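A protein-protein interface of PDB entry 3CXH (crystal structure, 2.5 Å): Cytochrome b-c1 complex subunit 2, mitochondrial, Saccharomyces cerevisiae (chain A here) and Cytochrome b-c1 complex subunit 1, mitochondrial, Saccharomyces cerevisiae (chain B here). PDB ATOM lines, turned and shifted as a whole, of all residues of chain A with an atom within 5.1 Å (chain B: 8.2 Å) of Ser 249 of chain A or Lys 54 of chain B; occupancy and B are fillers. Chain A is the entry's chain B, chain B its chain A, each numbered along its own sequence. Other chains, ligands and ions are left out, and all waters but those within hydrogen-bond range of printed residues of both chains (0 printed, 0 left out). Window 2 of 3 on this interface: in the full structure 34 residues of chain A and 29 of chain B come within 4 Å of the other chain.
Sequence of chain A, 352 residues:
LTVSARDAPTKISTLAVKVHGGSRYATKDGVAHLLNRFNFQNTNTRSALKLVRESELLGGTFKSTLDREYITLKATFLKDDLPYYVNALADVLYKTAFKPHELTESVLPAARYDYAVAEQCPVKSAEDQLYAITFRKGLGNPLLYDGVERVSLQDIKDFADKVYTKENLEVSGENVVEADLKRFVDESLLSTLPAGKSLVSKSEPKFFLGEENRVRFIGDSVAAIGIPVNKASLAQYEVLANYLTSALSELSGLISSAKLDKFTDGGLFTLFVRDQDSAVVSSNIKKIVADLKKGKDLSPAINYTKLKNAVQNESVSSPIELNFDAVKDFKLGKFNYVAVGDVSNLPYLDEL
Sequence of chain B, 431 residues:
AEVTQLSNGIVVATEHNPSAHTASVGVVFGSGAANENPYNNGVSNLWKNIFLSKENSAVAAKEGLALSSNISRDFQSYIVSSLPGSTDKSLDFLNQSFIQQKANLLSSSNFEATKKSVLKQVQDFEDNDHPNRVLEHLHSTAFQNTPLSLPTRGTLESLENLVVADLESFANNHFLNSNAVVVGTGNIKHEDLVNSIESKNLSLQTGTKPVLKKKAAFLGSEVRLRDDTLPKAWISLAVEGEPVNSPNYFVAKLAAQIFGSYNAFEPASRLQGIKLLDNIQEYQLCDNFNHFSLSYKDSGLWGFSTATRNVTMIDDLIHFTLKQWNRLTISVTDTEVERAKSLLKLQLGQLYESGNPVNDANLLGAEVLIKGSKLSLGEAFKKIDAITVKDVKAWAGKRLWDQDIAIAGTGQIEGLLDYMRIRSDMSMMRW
The backbone carbonyl oxygen (O) of Ser 53 of chain B is in hydrogen-bond range of the side-chain hydroxyl (OG) of Ser 57 of chain B (3.4 Å). OG of Ser 246 of chain A sits close to N of Leu 248 of chain A (3.5 Å). The backbone carbonyl oxygen (O) of Ser 246 of chain A sits at hydrogen-bond distance from the side-chain hydroxyl (OG) of Ser 252 of chain A (3.0 Å). OG of Ser 249 of chain A sits close to N of Leu 251 of chain A (3.3 Å). The side-chain hydroxyl (OG) of Ser 252 of chain A lies within hydrogen-bond range of the backbone carbonyl oxygen (O) of Ser 249 of chain A, 3.3 Å away.
Ala 247 of chain A touches Lys 54 of chain B. CB of Ala 247 of chain A touches CB of Ser 57 of chain B (3.6 Å). Ala 247 of chain A touches Ala 58 of chain B (CB to N, 3.3 Å). Ala 58 of chain B touches Leu 248 of chain A (O to CD2, 3.3 Å). CB of Ala 61 of chain B touches CG of Leu 248 of chain A, at 3.5 Å. Leu 248 of chain A touches Lys 62 of chain B. Lys 54 of chain B touches Ser 249 of chain A. Lys 54 of chain B touches Ser 252 of chain A.
Ser 249 of chain A touches just one residue of chain B: Lys 54 (3.9 Å). Of chain A, only Ala 247 (3.1 Å), Ser 249 (3.9 Å) and Ser 252 (3.8 Å) come within 4 Å of Lys 54 of chain B. Of the printed residues of chain B, Leu 248 of chain A touches Ala 58, Ala 61 and Lys 62. Of the printed residues of chain A, Ser 57 of chain B touches Ala 247 (3.6 Å). Of the printed residues of chain B, Ser 252 of chain A touches Lys 54. Printed residues of chain A within 4 Å of Lys 62 of chain B: Leu 248 (3.6 Å). Printed residues of chain B within 4 Å of Ala 247 of chain A: Lys 54, Ser 57 and Ala 58. The nearest printed residue of chain B that does not touch Ala 247 of chain A is Glu 55 of chain B (5.2 Å).
Along chain A the printed residues that touch a printed residue of chain B span positions 247 to 252. Hydrophobic or aromatic side chains of chain B within 4 Å of the printed part of chain A: Ala 58 and Ala 61. Among the printed residues, 8 pairs touch across the chains. Among the printed residues, no Asp or Glu carboxylate lies within 4 Å of a Lys or Arg side-chain nitrogen of the other chain.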
ATOM      1  N   TYR A 243     -32.681  15.931  -1.971  1.00  0.00           N
ATOM      2  CA  TYR A 243     -33.010  17.066  -2.824  1.00  0.00           C
ATOM      3  C   TYR A 243     -32.768  18.373  -2.065  1.00  0.00           C
ATOM      4  O   TYR A 243     -32.131  19.293  -2.584  1.00  0.00           O
ATOM      5  CB  TYR A 243     -34.475  16.972  -3.283  1.00  0.00           C
ATOM      6  CG  TYR A 243     -35.036  18.241  -3.897  1.00  0.00           C
ATOM      7  CD1 TYR A 243     -34.748  18.593  -5.220  1.00  0.00           C
ATOM      8  CD2 TYR A 243     -35.839  19.102  -3.146  1.00  0.00           C
ATOM      9  CE1 TYR A 243     -35.241  19.781  -5.778  1.00  0.00           C
ATOM     10  CE2 TYR A 243     -36.335  20.286  -3.689  1.00  0.00           C
ATOM     11  CZ  TYR A 243     -36.030  20.622  -5.003  1.00  0.00           C
ATOM     12  OH  TYR A 243     -36.491  21.813  -5.519  1.00  0.00           O
ATOM     13  N   LEU A 244     -33.248  18.425  -0.824  1.00  0.00           N
ATOM     14  CA  LEU A 244     -33.108  19.606   0.014  1.00  0.00           C
ATOM     15  C   LEU A 244     -31.682  19.841   0.503  1.00  0.00           C
ATOM     16  O   LEU A 244     -31.336  20.957   0.895  1.00  0.00           O
ATOM     17  CB  LEU A 244     -34.065  19.524   1.205  1.00  0.00           C
ATOM     18  CG  LEU A 244     -35.557  19.444   0.872  1.00  0.00           C
ATOM     19  CD1 LEU A 244     -36.378  19.249   2.136  1.00  0.00           C
ATOM     20  CD2 LEU A 244     -35.990  20.702   0.147  1.00  0.00           C
ATOM     21  N   SER A 246     -28.913  19.403  -1.389  1.00  0.00           N
ATOM     22  CA  SER A 246     -28.137  19.378  -2.627  1.00  0.00           C
ATOM     23  C   SER A 246     -28.299  20.707  -3.340  1.00  0.00           C
ATOM     24  O   SER A 246     -29.163  21.510  -2.981  1.00  0.00           O
ATOM     25  CB  SER A 246     -28.606  18.252  -3.554  1.00  0.00           C
ATOM     26  OG  SER A 246     -29.923  18.487  -4.035  1.00  0.00           O
ATOM     27  N   ALA A 247     -27.494  20.911  -4.377  1.00  0.00           N
ATOM     28  CA  ALA A 247     -27.531  22.148  -5.154  1.00  0.00           C
ATOM     29  C   ALA A 247     -28.783  22.299  -6.016  1.00  0.00           C
ATOM     30  O   ALA A 247     -29.020  23.366  -6.586  1.00  0.00           O
ATOM     31  CB  ALA A 247     -26.282  22.261  -6.009  1.00  0.00           C
ATOM     32  N   LEU A 248     -29.577  21.232  -6.109  1.00  0.00           N
ATOM     33  CA  LEU A 248     -30.811  21.245  -6.894  1.00  0.00           C
ATOM     34  C   LEU A 248     -31.913  22.089  -6.254  1.00  0.00           C
ATOM     35  O   LEU A 248     -32.817  22.564  -6.945  1.00  0.00           O
ATOM     36  CB  LEU A 248     -31.322  19.823  -7.137  1.00  0.00           C
ATOM     37  CG  LEU A 248     -30.426  18.939  -8.006  1.00  0.00           C
ATOM     38  CD1 LEU A 248     -31.123  17.627  -8.298  1.00  0.00           C
ATOM     39  CD2 LEU A 248     -30.099  19.650  -9.305  1.00  0.00           C
ATOM     40  N   SER A 249     -31.849  22.253  -4.937  1.00  0.00           N
ATOM     41  CA  SER A 249     -32.839  23.055  -4.235  1.00  0.00           C
ATOM     42  C   SER A 249     -32.296  24.440  -3.929  1.00  0.00           C
ATOM     43  O   SER A 249     -31.203  24.589  -3.380  1.00  0.00           O
ATOM     44  CB  SER A 249     -33.282  22.386  -2.940  1.00  0.00           C
ATOM     45  OG  SER A 249     -34.174  23.236  -2.242  1.00  0.00           O
ATOM     46  N   GLU A 250     -33.077  25.452  -4.288  1.00  0.00           N
ATOM     47  CA  GLU A 250     -32.694  26.834  -4.060  1.00  0.00           C
ATOM     48  C   GLU A 250     -32.921  27.219  -2.605  1.00  0.00           C
ATOM     49  O   GLU A 250     -33.102  28.394  -2.277  1.00  0.00           O
ATOM     50  CB  GLU A 250     -33.439  27.764  -5.029  1.00  0.00           C
ATOM     51  CG  GLU A 250     -32.884  27.703  -6.466  1.00  0.00           C
ATOM     52  CD  GLU A 250     -33.815  28.308  -7.520  1.00  0.00           C
ATOM     53  OE1 GLU A 250     -34.606  29.226  -7.193  1.00  0.00           O
ATOM     54  OE2 GLU A 250     -33.745  27.858  -8.689  1.00  0.00           O
ATOM     55  N   LEU A 251     -32.932  26.211  -1.738  1.00  0.00           N
ATOM     56  CA  LEU A 251     -33.094  26.436  -0.311  1.00  0.00           C
ATOM     57  C   LEU A 251     -32.306  25.432   0.533  1.00  0.00           C
ATOM     58  O   LEU A 251     -32.579  25.238   1.718  1.00  0.00           O
ATOM     59  CB  LEU A 251     -34.577  26.521   0.090  1.00  0.00           C
ATOM     60  CG  LEU A 251     -35.664  25.588  -0.443  1.00  0.00           C
ATOM     61  CD1 LEU A 251     -35.591  24.241   0.230  1.00  0.00           C
ATOM     62  CD2 LEU A 251     -37.004  26.221  -0.149  1.00  0.00           C
ATOM     63  N   SER A 252     -31.287  24.838  -0.083  1.00  0.00           N
ATOM     64  CA  SER A 252     -30.420  23.881   0.592  1.00  0.00           C
ATOM     65  C   SER A 252     -29.459  24.662   1.482  1.00  0.00           C
ATOM     66  O   SER A 252     -28.960  24.146   2.483  1.00  0.00           O
ATOM     67  CB  SER A 252     -29.635  23.052  -0.432  1.00  0.00           C
ATOM     68  OG  SER A 252     -28.766  23.858  -1.210  1.00  0.00           O
ATOM     69  N   GLY A 253     -29.197  25.907   1.089  1.00  0.00           N
ATOM     70  CA  GLY A 253     -28.313  26.770   1.849  1.00  0.00           C
ATOM     71  C   GLY A 253     -29.061  27.485   2.959  1.00  0.00           C
ATOM     72  O   GLY A 253     -28.498  28.305   3.681  1.00  0.00           O
ATOM     73  N   ASN B  49     -13.173  25.136  -3.461  1.00  0.00           N
ATOM     74  CA  ASN B  49     -14.508  25.634  -3.196  1.00  0.00           C
ATOM     75  C   ASN B  49     -15.320  26.119  -4.387  1.00  0.00           C
ATOM     76  O   ASN B  49     -16.555  26.128  -4.315  1.00  0.00           O
ATOM     77  CB  ASN B  49     -14.485  26.674  -2.078  1.00  0.00           C
ATOM     78  CG  ASN B  49     -14.466  26.038  -0.705  1.00  0.00           C
ATOM     79  OD1 ASN B  49     -15.513  25.756  -0.127  1.00  0.00           O
ATOM     80  ND2 ASN B  49     -13.272  25.788  -0.185  1.00  0.00           N
ATOM     81  N   ILE B  50     -14.658  26.558  -5.459  1.00  0.00           N
ATOM     82  CA  ILE B  50     -15.416  26.988  -6.633  1.00  0.00           C
ATOM     83  C   ILE B  50     -15.852  25.752  -7.417  1.00  0.00           C
ATOM     84  O   ILE B  50     -16.881  25.772  -8.092  1.00  0.00           O
ATOM     85  CB  ILE B  50     -14.650  27.962  -7.554  1.00  0.00           C
ATOM     86  CG1 ILE B  50     -13.358  27.338  -8.049  1.00  0.00           C
ATOM     87  CG2 ILE B  50     -14.398  29.280  -6.854  1.00  0.00           C
ATOM     88  CD1 ILE B  50     -12.638  28.235  -9.004  1.00  0.00           C
ATOM     89  N   PHE B  51     -15.075  24.676  -7.293  1.00  0.00           N
ATOM     90  CA  PHE B  51     -15.378  23.402  -7.941  1.00  0.00           C
ATOM     91  C   PHE B  51     -16.587  22.760  -7.252  1.00  0.00           C
ATOM     92  O   PHE B  51     -17.257  21.908  -7.828  1.00  0.00           O
ATOM     93  CB  PHE B  51     -14.168  22.461  -7.857  1.00  0.00           C
ATOM     94  CG  PHE B  51     -14.430  21.062  -8.374  1.00  0.00           C
ATOM     95  CD1 PHE B  51     -14.328  20.774  -9.730  1.00  0.00           C
ATOM     96  CD2 PHE B  51     -14.765  20.031  -7.498  1.00  0.00           C
ATOM     97  CE1 PHE B  51     -14.555  19.480 -10.207  1.00  0.00           C
ATOM     98  CE2 PHE B  51     -14.993  18.734  -7.967  1.00  0.00           C
ATOM     99  CZ  PHE B  51     -14.886  18.461  -9.323  1.00  0.00           C
ATOM    100  N   LEU B  52     -16.848  23.179  -6.013  1.00  0.00           N
ATOM    101  CA  LEU B  52     -17.966  22.671  -5.216  1.00  0.00           C
ATOM    102  C   LEU B  52     -19.086  23.703  -5.095  1.00  0.00           C
ATOM    103  O   LEU B  52     -19.980  23.559  -4.265  1.00  0.00           O
ATOM    104  CB  LEU B  52     -17.489  22.288  -3.810  1.00  0.00           C
ATOM    105  CG  LEU B  52     -16.511  21.124  -3.653  1.00  0.00           C
ATOM    106  CD1 LEU B  52     -15.917  21.128  -2.255  1.00  0.00           C
ATOM    107  CD2 LEU B  52     -17.224  19.819  -3.930  1.00  0.00           C
ATOM    108  N   SER B  53     -19.020  24.753  -5.909  1.00  0.00           N
ATOM    109  CA  SER B  53     -20.032  25.807  -5.897  1.00  0.00           C
ATOM    110  C   SER B  53     -21.413  25.247  -6.272  1.00  0.00           C
ATOM    111  O   SER B  53     -21.509  24.310  -7.068  1.00  0.00           O
ATOM    112  CB  SER B  53     -19.623  26.910  -6.868  1.00  0.00           C
ATOM    113  OG  SER B  53     -20.560  27.966  -6.839  1.00  0.00           O
ATOM    114  N   LYS B  54     -22.475  25.829  -5.709  1.00  0.00           N
ATOM    115  CA  LYS B  54     -23.845  25.367  -5.966  1.00  0.00           C
ATOM    116  C   LYS B  54     -24.163  25.187  -7.448  1.00  0.00           C
ATOM    117  O   LYS B  54     -24.762  24.188  -7.847  1.00  0.00           O
ATOM    118  CB  LYS B  54     -24.880  26.307  -5.332  1.00  0.00           C
ATOM    119  CG  LYS B  54     -26.329  25.864  -5.578  1.00  0.00           C
ATOM    120  CD  LYS B  54     -27.376  26.796  -4.963  1.00  0.00           C
ATOM    121  CE  LYS B  54     -27.489  26.629  -3.452  1.00  0.00           C
ATOM    122  NZ  LYS B  54     -28.586  27.466  -2.872  1.00  0.00           N
ATOM    123  N   GLU B  55     -23.742  26.151  -8.256  1.00  0.00           N
ATOM    124  CA  GLU B  55     -23.978  26.120  -9.693  1.00  0.00           C
ATOM    125  C   GLU B  55     -23.385  24.863 -10.328  1.00  0.00           C
ATOM    126  O   GLU B  55     -24.104  24.064 -10.924  1.00  0.00           O
ATOM    127  CB  GLU B  55     -23.390  27.381 -10.336  1.00  0.00           C
ATOM    128  CG  GLU B  55     -23.871  28.688  -9.682  1.00  0.00           C
ATOM    129  CD  GLU B  55     -23.144  29.937 -10.186  1.00  0.00           C
ATOM    130  OE1 GLU B  55     -22.133  29.805 -10.920  1.00  0.00           O
ATOM    131  OE2 GLU B  55     -23.585  31.058  -9.835  1.00  0.00           O
ATOM    132  N   ASN B  56     -22.083  24.661 -10.146  1.00  0.00           N
ATOM    133  CA  ASN B  56     -21.403  23.500 -10.712  1.00  0.00           C
ATOM    134  C   ASN B  56     -21.830  22.174 -10.082  1.00  0.00           C
ATOM    135  O   ASN B  56     -21.485  21.104 -10.587  1.00  0.00           O
ATOM    136  CB  ASN B  56     -19.887  23.660 -10.590  1.00  0.00           C
ATOM    137  CG  ASN B  56     -19.126  22.691 -11.479  1.00  0.00           C
ATOM    138  OD1 ASN B  56     -19.715  22.007 -12.310  1.00  0.00           O
ATOM    139  ND2 ASN B  56     -17.811  22.640 -11.317  1.00  0.00           N
ATOM    140  N   SER B  57     -22.560  22.241  -8.972  1.00  0.00           N
ATOM    141  CA  SER B  57     -23.017  21.032  -8.294  1.00  0.00           C
ATOM    142  C   SER B  57     -24.406  20.620  -8.733  1.00  0.00           C
ATOM    143  O   SER B  57     -24.712  19.429  -8.790  1.00  0.00           O
ATOM    144  CB  SER B  57     -22.960  21.189  -6.771  1.00  0.00           C
ATOM    145  OG  SER B  57     -21.643  20.975  -6.290  1.00  0.00           O
ATOM    146  N   ALA B  58     -25.247  21.608  -9.029  1.00  0.00           N
ATOM    147  CA  ALA B  58     -26.614  21.359  -9.491  1.00  0.00           C
ATOM    148  C   ALA B  58     -26.536  20.593 -10.813  1.00  0.00           C
ATOM    149  O   ALA B  58     -27.323  19.683 -11.070  1.00  0.00           O
ATOM    150  CB  ALA B  58     -27.359  22.686  -9.678  1.00  0.00           C
ATOM    151  N   VAL B  59     -25.539  20.943 -11.621  1.00  0.00           N
ATOM    152  CA  VAL B  59     -25.309  20.303 -12.905  1.00  0.00           C
ATOM    153  C   VAL B  59     -25.005  18.823 -12.673  1.00  0.00           C
ATOM    154  O   VAL B  59     -25.696  17.952 -13.200  1.00  0.00           O
ATOM    155  CB  VAL B  59     -24.138  20.993 -13.656  1.00  0.00           C
ATOM    156  CG1 VAL B  59     -23.817  20.262 -14.955  1.00  0.00           C
ATOM    157  CG2 VAL B  59     -24.488  22.449 -13.937  1.00  0.00           C
ATOM    158  N   ALA B  60     -24.010  18.552 -11.832  1.00  0.00           N
ATOM    159  CA  ALA B  60     -23.603  17.189 -11.501  1.00  0.00           C
ATOM    160  C   ALA B  60     -24.695  16.363 -10.813  1.00  0.00           C
ATOM    161  O   ALA B  60     -24.731  15.142 -10.950  1.00  0.00           O
ATOM    162  CB  ALA B  60     -22.362  17.226 -10.632  1.00  0.00           C
ATOM    163  N   ALA B  61     -25.568  17.026 -10.062  1.00  0.00           N
ATOM    164  CA  ALA B  61     -26.649  16.340  -9.359  1.00  0.00           C
ATOM    165  C   ALA B  61     -27.678  15.733 -10.320  1.00  0.00           C
ATOM    166  O   ALA B  61     -28.108  14.591 -10.136  1.00  0.00           O
ATOM    167  CB  ALA B  61     -27.325  17.290  -8.388  1.00  0.00           C
ATOM    168  N   LYS B  62     -28.062  16.497 -11.342  1.00  0.00           N
ATOM    169  CA  LYS B  62     -29.029  16.035 -12.345  1.00  0.00           C
ATOM    170  C   LYS B  62     -28.523  14.797 -13.083  1.00  0.00           C
ATOM    171  O   LYS B  62     -29.308  13.932 -13.487  1.00  0.00           O
ATOM    172  CB  LYS B  62     -29.344  17.161 -13.339  1.00  0.00           C
ATOM    173  CG  LYS B  62     -30.270  18.231 -12.762  1.00  0.00           C
ATOM    174  CD  LYS B  62     -30.012  19.613 -13.343  1.00  0.00           C
ATOM    175  CE  LYS B  62     -30.867  20.655 -12.632  1.00  0.00           C
ATOM    176  NZ  LYS B  62     -30.434  22.049 -12.928  1.00  0.00           N
ATOM    177  N   LEU B  67     -19.890  15.520  -5.928  1.00  0.00           N
ATOM    178  CA  LEU B  67     -18.590  16.196  -6.032  1.00  0.00           C
ATOM    179  C   LEU B  67     -17.705  16.195  -4.778  1.00  0.00           C
ATOM    180  O   LEU B  67     -18.179  16.467  -3.671  1.00  0.00           O
ATOM    181  CB  LEU B  67     -18.798  17.634  -6.510  1.00  0.00           C
ATOM    182  CG  LEU B  67     -19.488  17.794  -7.868  1.00  0.00           C
ATOM    183  CD1 LEU B  67     -19.639  19.270  -8.199  1.00  0.00           C
ATOM    184  CD2 LEU B  67     -18.683  17.064  -8.944  1.00  0.00           C
ATOM    185  N   LEU B 105     -17.253  28.989 -13.941  1.00  0.00           N
ATOM    186  CA  LEU B 105     -16.926  28.858 -12.528  1.00  0.00           C
ATOM    187  C   LEU B 105     -16.225  30.110 -12.022  1.00  0.00           C
ATOM    188  O   LEU B 105     -16.324  30.449 -10.844  1.00  0.00           O
ATOM    189  CB  LEU B 105     -16.034  27.637 -12.301  1.00  0.00           C
ATOM    190  CG  LEU B 105     -16.624  26.297 -12.735  1.00  0.00           C
ATOM    191  CD1 LEU B 105     -15.666  25.169 -12.397  1.00  0.00           C
ATOM    192  CD2 LEU B 105     -17.962  26.092 -12.056  1.00  0.00           C
ATOM    193  N   ASN B 110     -19.965  34.201  -9.245  1.00  0.00           N
ATOM    194  CA  ASN B 110     -19.570  32.962  -8.582  1.00  0.00           C
ATOM    195  C   ASN B 110     -18.327  33.146  -7.726  1.00  0.00           C
ATOM    196  O   ASN B 110     -18.300  32.726  -6.567  1.00  0.00           O
ATOM    197  CB  ASN B 110     -19.327  31.852  -9.606  1.00  0.00           C
ATOM    198  CG  ASN B 110     -19.422  30.464  -8.996  1.00  0.00           C
ATOM    199  OD1 ASN B 110     -20.145  30.257  -8.023  1.00  0.00           O
ATOM    200  ND2 ASN B 110     -18.709  29.504  -9.575  1.00  0.00           N
ATOM    201  N   ALA B 113     -18.985  35.073  -4.518  1.00  0.00           N
ATOM    202  CA  ALA B 113     -19.771  34.290  -3.566  1.00  0.00           C
ATOM    203  C   ALA B 113     -18.905  33.240  -2.874  1.00  0.00           C
ATOM    204  O   ALA B 113     -19.024  33.026  -1.669  1.00  0.00           O
ATOM    205  CB  ALA B 113     -20.945  33.625  -4.270  1.00  0.00           C
ATOM    206  N   THR B 114     -18.033  32.598  -3.649  1.00  0.00           N
ATOM    207  CA  THR B 114     -17.135  31.567  -3.140  1.00  0.00           C
ATOM    208  C   THR B 114     -16.071  32.163  -2.220  1.00  0.00           C
ATOM    209  O   THR B 114     -15.759  31.601  -1.172  1.00  0.00           O
ATOM    210  CB  THR B 114     -16.417  30.839  -4.294  1.00  0.00           C
ATOM    211  OG1 THR B 114     -17.385  30.321  -5.211  1.00  0.00           O
ATOM    212  CG2 THR B 114     -15.585  29.690  -3.761  1.00  0.00           C
